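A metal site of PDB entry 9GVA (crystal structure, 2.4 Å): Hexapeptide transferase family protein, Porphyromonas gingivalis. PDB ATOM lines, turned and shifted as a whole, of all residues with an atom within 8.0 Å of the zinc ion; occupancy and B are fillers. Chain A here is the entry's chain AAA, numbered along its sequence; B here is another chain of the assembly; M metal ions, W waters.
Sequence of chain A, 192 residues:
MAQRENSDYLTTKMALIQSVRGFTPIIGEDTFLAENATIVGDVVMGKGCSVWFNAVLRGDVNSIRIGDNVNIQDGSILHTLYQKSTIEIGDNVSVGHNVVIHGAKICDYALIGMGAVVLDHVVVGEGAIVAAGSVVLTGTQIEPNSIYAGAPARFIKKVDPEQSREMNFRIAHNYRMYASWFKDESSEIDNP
The zinc ion is bound by ND1 of His 79, NE2 of His 97 of chain B, NE2 of His 102 and water W1.
Gln 73 of chain B touches the zinc ion (OE1 to ZN, 3.97 Å).
Tyr 175 of chain B touches the zinc ion.
The nearest printed residue that does not touch the zinc ion is Thr 80 (4.04 Å).
O of Ile 101 sits at hydrogen-bond distance from N of His 79, 2.9 Å away.
The side-chain amide oxygen (OE1) of Gln 73 of chain B lies close to the backbone NH (N) of His 97 of chain B (3.3 Å).
The backbone NH (N) of Gly 103 is in hydrogen-bond range of the backbone carbonyl oxygen (O) of His 79 (2.9 Å).
OH of Tyr 175 of chain B is in hydrogen-bond range of NH2 of Arg 58 (2.8 Å).
A ring nitrogen (NE2) of His 79 sits close to the guanidinium group (NH1) of Arg 58.
ND1 of His 102 sits at hydrogen-bond distance from OD2 of Asp 120 (2.8 Å).
The side-chain hydroxyl (OH) of Tyr 175 of chain B sits close to the side-chain amide oxygen (OE1) of Gln 73 of chain B (3.3 Å).
OD1 of Asp 74 of chain B lies within hydrogen-bond range of ND1 of His 97 of chain B.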
ATOM      1  N   ARG A  58     -16.131 -16.285 -28.760  1.00  0.00           N
ATOM      2  CA  ARG A  58     -16.773 -17.595 -28.569  1.00  0.00           C
ATOM      3  C   ARG A  58     -18.140 -17.602 -29.274  1.00  0.00           C
ATOM      4  O   ARG A  58     -19.105 -17.166 -28.673  1.00  0.00           O
ATOM      5  CB  ARG A  58     -16.828 -17.983 -27.089  1.00  0.00           C
ATOM      6  CG  ARG A  58     -17.703 -19.204 -26.881  1.00  0.00           C
ATOM      7  CD  ARG A  58     -17.267 -20.213 -25.869  1.00  0.00           C
ATOM      8  NE  ARG A  58     -17.622 -19.883 -24.538  1.00  0.00           N
ATOM      9  CZ  ARG A  58     -18.561 -20.409 -23.744  1.00  0.00           C
ATOM     10  NH1 ARG A  58     -19.431 -21.327 -24.120  1.00  0.00           N
ATOM     11  NH2 ARG A  58     -18.614 -19.952 -22.507  1.00  0.00           N
ATOM     12  N   ASP A  60     -20.225 -20.096 -30.122  1.00  0.00           N
ATOM     13  CA  ASP A  60     -20.722 -21.474 -29.982  1.00  0.00           C
ATOM     14  C   ASP A  60     -22.257 -21.441 -29.886  1.00  0.00           C
ATOM     15  O   ASP A  60     -22.851 -22.298 -30.518  1.00  0.00           O
ATOM     16  CB  ASP A  60     -20.046 -22.172 -28.807  1.00  0.00           C
ATOM     17  CG  ASP A  60     -20.176 -21.527 -27.428  1.00  0.00           C
ATOM     18  OD1 ASP A  60     -20.622 -20.358 -27.331  1.00  0.00           O
ATOM     19  OD2 ASP A  60     -19.810 -22.214 -26.463  1.00  0.00           O
ATOM     20  N   VAL A  61     -22.863 -20.522 -29.131  1.00  0.00           N
ATOM     21  CA  VAL A  61     -24.328 -20.589 -28.816  1.00  0.00           C
ATOM     22  C   VAL A  61     -25.125 -19.597 -29.663  1.00  0.00           C
ATOM     23  O   VAL A  61     -26.344 -19.697 -29.647  1.00  0.00           O
ATOM     24  CB  VAL A  61     -24.607 -20.358 -27.328  1.00  0.00           C
ATOM     25  CG1 VAL A  61     -23.917 -21.413 -26.507  1.00  0.00           C
ATOM     26  CG2 VAL A  61     -24.183 -18.970 -26.877  1.00  0.00           C
ATOM     27  N   ILE A  77     -13.458 -10.998 -23.809  1.00  0.00           N
ATOM     28  CA  ILE A  77     -14.344 -12.155 -24.033  1.00  0.00           C
ATOM     29  C   ILE A  77     -15.566 -11.621 -24.745  1.00  0.00           C
ATOM     30  O   ILE A  77     -16.186 -10.680 -24.173  1.00  0.00           O
ATOM     31  CB  ILE A  77     -14.758 -12.825 -22.725  1.00  0.00           C
ATOM     32  CG1 ILE A  77     -13.575 -13.098 -21.792  1.00  0.00           C
ATOM     33  CG2 ILE A  77     -15.561 -14.091 -23.038  1.00  0.00           C
ATOM     34  CD1 ILE A  77     -12.585 -14.064 -22.310  1.00  0.00           C
ATOM     35  N   LEU A  78     -15.883 -12.237 -25.886  1.00  0.00           N
ATOM     36  CA  LEU A  78     -17.105 -11.975 -26.665  1.00  0.00           C
ATOM     37  C   LEU A  78     -17.942 -13.247 -26.627  1.00  0.00           C
ATOM     38  O   LEU A  78     -17.458 -14.329 -27.012  1.00  0.00           O
ATOM     39  CB  LEU A  78     -16.755 -11.522 -28.080  1.00  0.00           C
ATOM     40  CG  LEU A  78     -16.547 -10.009 -28.242  1.00  0.00           C
ATOM     41  CD1 LEU A  78     -15.334  -9.532 -27.462  1.00  0.00           C
ATOM     42  CD2 LEU A  78     -16.384  -9.667 -29.699  1.00  0.00           C
ATOM     43  N   HIS A  79     -19.139 -13.131 -26.072  1.00  0.00           N
ATOM     44  CA  HIS A  79     -20.068 -14.271 -25.973  1.00  0.00           C
ATOM     45  C   HIS A  79     -21.486 -13.771 -26.107  1.00  0.00           C
ATOM     46  O   HIS A  79     -21.680 -12.553 -26.204  1.00  0.00           O
ATOM     47  CB  HIS A  79     -19.750 -15.045 -24.691  1.00  0.00           C
ATOM     48  CG  HIS A  79     -20.265 -16.441 -24.724  1.00  0.00           C
ATOM     49  ND1 HIS A  79     -20.958 -16.986 -23.652  1.00  0.00           N
ATOM     50  CD2 HIS A  79     -20.247 -17.380 -25.699  1.00  0.00           C
ATOM     51  CE1 HIS A  79     -21.359 -18.214 -23.975  1.00  0.00           C
ATOM     52  NE2 HIS A  79     -20.912 -18.500 -25.216  1.00  0.00           N
ATOM     53  N   THR A  80     -22.431 -14.709 -26.143  1.00  0.00           N
ATOM     54  CA  THR A  80     -23.879 -14.487 -26.406  1.00  0.00           C
ATOM     55  C   THR A  80     -24.687 -15.417 -25.519  1.00  0.00           C
ATOM     56  O   THR A  80     -24.116 -16.378 -25.044  1.00  0.00           O
ATOM     57  CB  THR A  80     -24.164 -14.736 -27.895  1.00  0.00           C
ATOM     58  OG1 THR A  80     -23.940 -16.138 -28.091  1.00  0.00           O
ATOM     59  CG2 THR A  80     -23.308 -13.899 -28.816  1.00  0.00           C
ATOM     60  N   LEU A  81     -25.961 -15.152 -25.340  1.00  0.00           N
ATOM     61  CA  LEU A  81     -26.922 -16.129 -24.757  1.00  0.00           C
ATOM     62  C   LEU A  81     -27.513 -17.023 -25.877  1.00  0.00           C
ATOM     63  O   LEU A  81     -27.991 -16.487 -26.867  1.00  0.00           O
ATOM     64  CB  LEU A  81     -28.013 -15.330 -24.062  1.00  0.00           C
ATOM     65  CG  LEU A  81     -27.572 -14.569 -22.821  1.00  0.00           C
ATOM     66  CD1 LEU A  81     -28.647 -13.565 -22.414  1.00  0.00           C
ATOM     67  CD2 LEU A  81     -27.300 -15.539 -21.670  1.00  0.00           C
ATOM     68  N   TYR A  82     -27.424 -18.343 -25.723  1.00  0.00           N
ATOM     69  CA  TYR A  82     -28.032 -19.359 -26.628  1.00  0.00           C
ATOM     70  C   TYR A  82     -29.462 -19.008 -27.046  1.00  0.00           C
ATOM     71  O   TYR A  82     -30.363 -18.901 -26.159  1.00  0.00           O
ATOM     72  CB  TYR A  82     -28.022 -20.715 -25.924  1.00  0.00           C
ATOM     73  CG  TYR A  82     -28.428 -21.871 -26.794  1.00  0.00           C
ATOM     74  CD1 TYR A  82     -27.986 -21.990 -28.097  1.00  0.00           C
ATOM     75  CD2 TYR A  82     -29.214 -22.890 -26.265  1.00  0.00           C
ATOM     76  CE1 TYR A  82     -28.360 -23.064 -28.891  1.00  0.00           C
ATOM     77  CE2 TYR A  82     -29.570 -23.981 -27.033  1.00  0.00           C
ATOM     78  CZ  TYR A  82     -29.134 -24.062 -28.335  1.00  0.00           C
ATOM     79  OH  TYR A  82     -29.483 -25.153 -29.040  1.00  0.00           O
ATOM     80  N   SER A  85     -29.428 -13.885 -27.643  1.00  0.00           N
ATOM     81  CA  SER A  85     -28.678 -12.630 -27.872  1.00  0.00           C
ATOM     82  C   SER A  85     -27.592 -12.895 -28.898  1.00  0.00           C
ATOM     83  O   SER A  85     -27.165 -14.049 -28.939  1.00  0.00           O
ATOM     84  CB  SER A  85     -28.118 -12.045 -26.564  1.00  0.00           C
ATOM     85  OG  SER A  85     -27.053 -12.854 -26.047  1.00  0.00           O
ATOM     86  N   VAL A 100     -15.743  -7.743 -21.095  1.00  0.00           N
ATOM     87  CA  VAL A 100     -16.721  -8.788 -21.521  1.00  0.00           C
ATOM     88  C   VAL A 100     -17.833  -8.135 -22.335  1.00  0.00           C
ATOM     89  O   VAL A 100     -18.395  -7.152 -21.872  1.00  0.00           O
ATOM     90  CB  VAL A 100     -17.284  -9.581 -20.343  1.00  0.00           C
ATOM     91  CG1 VAL A 100     -18.213 -10.693 -20.852  1.00  0.00           C
ATOM     92  CG2 VAL A 100     -16.137 -10.162 -19.492  1.00  0.00           C
ATOM     93  N   ILE A 101     -18.013  -8.568 -23.581  1.00  0.00           N
ATOM     94  CA  ILE A 101     -19.164  -8.166 -24.419  1.00  0.00           C
ATOM     95  C   ILE A 101     -20.066  -9.397 -24.533  1.00  0.00           C
ATOM     96  O   ILE A 101     -19.619 -10.409 -25.063  1.00  0.00           O
ATOM     97  CB  ILE A 101     -18.715  -7.571 -25.756  1.00  0.00           C
ATOM     98  CG1 ILE A 101     -18.081  -6.205 -25.476  1.00  0.00           C
ATOM     99  CG2 ILE A 101     -19.868  -7.404 -26.753  1.00  0.00           C
ATOM    100  CD1 ILE A 101     -17.129  -5.787 -26.500  1.00  0.00           C
ATOM    101  N   HIS A 102     -21.264  -9.297 -23.985  1.00  0.00           N
ATOM    102  CA  HIS A 102     -22.226 -10.408 -23.958  1.00  0.00           C
ATOM    103  C   HIS A 102     -23.507  -9.980 -24.702  1.00  0.00           C
ATOM    104  O   HIS A 102     -24.276  -9.265 -24.120  1.00  0.00           O
ATOM    105  CB  HIS A 102     -22.495 -10.843 -22.498  1.00  0.00           C
ATOM    106  CG  HIS A 102     -22.718 -12.312 -22.370  1.00  0.00           C
ATOM    107  ND1 HIS A 102     -23.938 -12.880 -22.630  1.00  0.00           N
ATOM    108  CD2 HIS A 102     -21.860 -13.331 -22.132  1.00  0.00           C
ATOM    109  CE1 HIS A 102     -23.855 -14.193 -22.479  1.00  0.00           C
ATOM    110  NE2 HIS A 102     -22.583 -14.498 -22.161  1.00  0.00           N
ATOM    111  N   GLY A 103     -23.698 -10.431 -25.934  1.00  0.00           N
ATOM    112  CA  GLY A 103     -24.949 -10.273 -26.700  1.00  0.00           C
ATOM    113  C   GLY A 103     -25.291  -8.806 -26.937  1.00  0.00           C
ATOM    114  O   GLY A 103     -26.449  -8.459 -26.860  1.00  0.00           O
ATOM    115  N   ASP A 120     -26.390  -8.229 -22.282  1.00  0.00           N
ATOM    116  CA  ASP A 120     -27.167  -8.579 -23.505  1.00  0.00           C
ATOM    117  C   ASP A 120     -28.183  -7.477 -23.821  1.00  0.00           C
ATOM    118  O   ASP A 120     -28.666  -6.786 -22.883  1.00  0.00           O
ATOM    119  CB  ASP A 120     -27.725  -9.992 -23.352  1.00  0.00           C
ATOM    120  CG  ASP A 120     -26.644 -10.986 -22.932  1.00  0.00           C
ATOM    121  OD1 ASP A 120     -26.284 -11.000 -21.721  1.00  0.00           O
ATOM    122  OD2 ASP A 120     -26.135 -11.715 -23.806  1.00  0.00           O
ATOM    123  N   GLN B  73     -16.320 -20.342 -16.627  1.00  0.00           N
ATOM    124  CA  GLN B  73     -16.389 -19.762 -17.991  1.00  0.00           C
ATOM    125  C   GLN B  73     -15.082 -19.030 -18.291  1.00  0.00           C
ATOM    126  O   GLN B  73     -14.176 -19.033 -17.423  1.00  0.00           O
ATOM    127  CB  GLN B  73     -17.616 -18.884 -18.127  1.00  0.00           C
ATOM    128  CG  GLN B  73     -18.905 -19.657 -18.198  1.00  0.00           C
ATOM    129  CD  GLN B  73     -20.104 -18.744 -18.060  1.00  0.00           C
ATOM    130  OE1 GLN B  73     -20.062 -17.582 -18.492  1.00  0.00           O
ATOM    131  NE2 GLN B  73     -21.158 -19.300 -17.457  1.00  0.00           N
ATOM    132  N   ASP B  74     -15.014 -18.466 -19.493  1.00  0.00           N
ATOM    133  CA  ASP B  74     -13.753 -18.037 -20.157  1.00  0.00           C
ATOM    134  C   ASP B  74     -13.155 -16.925 -19.309  1.00  0.00           C
ATOM    135  O   ASP B  74     -13.890 -16.076 -18.829  1.00  0.00           O
ATOM    136  CB  ASP B  74     -13.984 -17.619 -21.611  1.00  0.00           C
ATOM    137  CG  ASP B  74     -15.004 -18.501 -22.342  1.00  0.00           C
ATOM    138  OD1 ASP B  74     -16.236 -18.336 -22.083  1.00  0.00           O
ATOM    139  OD2 ASP B  74     -14.566 -19.353 -23.151  1.00  0.00           O
ATOM    140  N   GLY B  96     -19.394 -17.205 -14.180  1.00  0.00           N
ATOM    141  CA  GLY B  96     -19.381 -16.343 -15.378  1.00  0.00           C
ATOM    142  C   GLY B  96     -17.991 -15.985 -15.898  1.00  0.00           C
ATOM    143  O   GLY B  96     -16.967 -16.238 -15.183  1.00  0.00           O
ATOM    144  N   HIS B  97     -17.950 -15.421 -17.113  1.00  0.00           N
ATOM    145  CA  HIS B  97     -16.707 -15.006 -17.807  1.00  0.00           C
ATOM    146  C   HIS B  97     -15.948 -14.000 -16.926  1.00  0.00           C
ATOM    147  O   HIS B  97     -16.616 -13.123 -16.332  1.00  0.00           O
ATOM    148  CB  HIS B  97     -17.031 -14.423 -19.187  1.00  0.00           C
ATOM    149  CG  HIS B  97     -18.023 -15.151 -20.026  1.00  0.00           C
ATOM    150  ND1 HIS B  97     -17.678 -16.230 -20.808  1.00  0.00           N
ATOM    151  CD2 HIS B  97     -19.335 -14.899 -20.273  1.00  0.00           C
ATOM    152  CE1 HIS B  97     -18.749 -16.626 -21.480  1.00  0.00           C
ATOM    153  NE2 HIS B  97     -19.769 -15.837 -21.159  1.00  0.00           N
ATOM    154  N   MET B 114     -20.791 -12.602 -14.666  1.00  0.00           N
ATOM    155  CA  MET B 114     -19.546 -12.299 -15.373  1.00  0.00           C
ATOM    156  C   MET B 114     -18.957 -11.011 -14.798  1.00  0.00           C
ATOM    157  O   MET B 114     -19.728 -10.088 -14.413  1.00  0.00           O
ATOM    158  CB  MET B 114     -19.796 -12.174 -16.869  1.00  0.00           C
ATOM    159  CG  MET B 114     -20.780 -11.116 -17.234  1.00  0.00           C
ATOM    160  SD  MET B 114     -21.194 -11.324 -18.953  1.00  0.00           S
ATOM    161  CE  MET B 114     -22.694 -12.292 -18.758  1.00  0.00           C
ATOM    162  N   TYR B 175     -24.953 -25.606 -20.308  1.00  0.00           N
ATOM    163  CA  TYR B 175     -23.474 -25.497 -20.414  1.00  0.00           C
ATOM    164  C   TYR B 175     -22.885 -26.888 -20.680  1.00  0.00           C
ATOM    165  O   TYR B 175     -21.914 -26.988 -21.489  1.00  0.00           O
ATOM    166  CB  TYR B 175     -22.867 -24.764 -19.201  1.00  0.00           C
ATOM    167  CG  TYR B 175     -22.338 -23.408 -19.571  1.00  0.00           C
ATOM    168  CD1 TYR B 175     -21.041 -23.293 -20.070  1.00  0.00           C
ATOM    169  CD2 TYR B 175     -23.149 -22.277 -19.604  1.00  0.00           C
ATOM    170  CE1 TYR B 175     -20.523 -22.067 -20.470  1.00  0.00           C
ATOM    171  CE2 TYR B 175     -22.668 -21.059 -20.048  1.00  0.00           C
ATOM    172  CZ  TYR B 175     -21.339 -20.956 -20.468  1.00  0.00           C
ATOM    173  OH  TYR B 175     -20.824 -19.753 -20.842  1.00  0.00           O
ATOM    174  N   TYR B 178     -23.400 -27.315 -24.364  1.00  0.00           N
ATOM    175  CA  TYR B 178     -22.419 -26.511 -25.140  1.00  0.00           C
ATOM    176  C   TYR B 178     -21.055 -27.193 -25.112  1.00  0.00           C
ATOM    177  O   TYR B 178     -20.370 -27.203 -26.128  1.00  0.00           O
ATOM    178  CB  TYR B 178     -22.228 -25.075 -24.632  1.00  0.00           C
ATOM    179  CG  TYR B 178     -23.489 -24.300 -24.331  1.00  0.00           C
ATOM    180  CD1 TYR B 178     -24.690 -24.555 -24.979  1.00  0.00           C
ATOM    181  CD2 TYR B 178     -23.475 -23.322 -23.363  1.00  0.00           C
ATOM    182  CE1 TYR B 178     -25.851 -23.848 -24.651  1.00  0.00           C
ATOM    183  CE2 TYR B 178     -24.608 -22.613 -23.023  1.00  0.00           C
ATOM    184  CZ  TYR B 178     -25.804 -22.873 -23.658  1.00  0.00           C
ATOM    185  OH  TYR B 178     -26.891 -22.121 -23.272  1.00  0.00           O
HETATM  186 ZN    ZN M   1     -21.572 -16.236 -21.913  1.00  0.00          ZN
HETATM  187  O   HOH W   1     -22.771 -17.748 -20.816  1.00  0.00           O
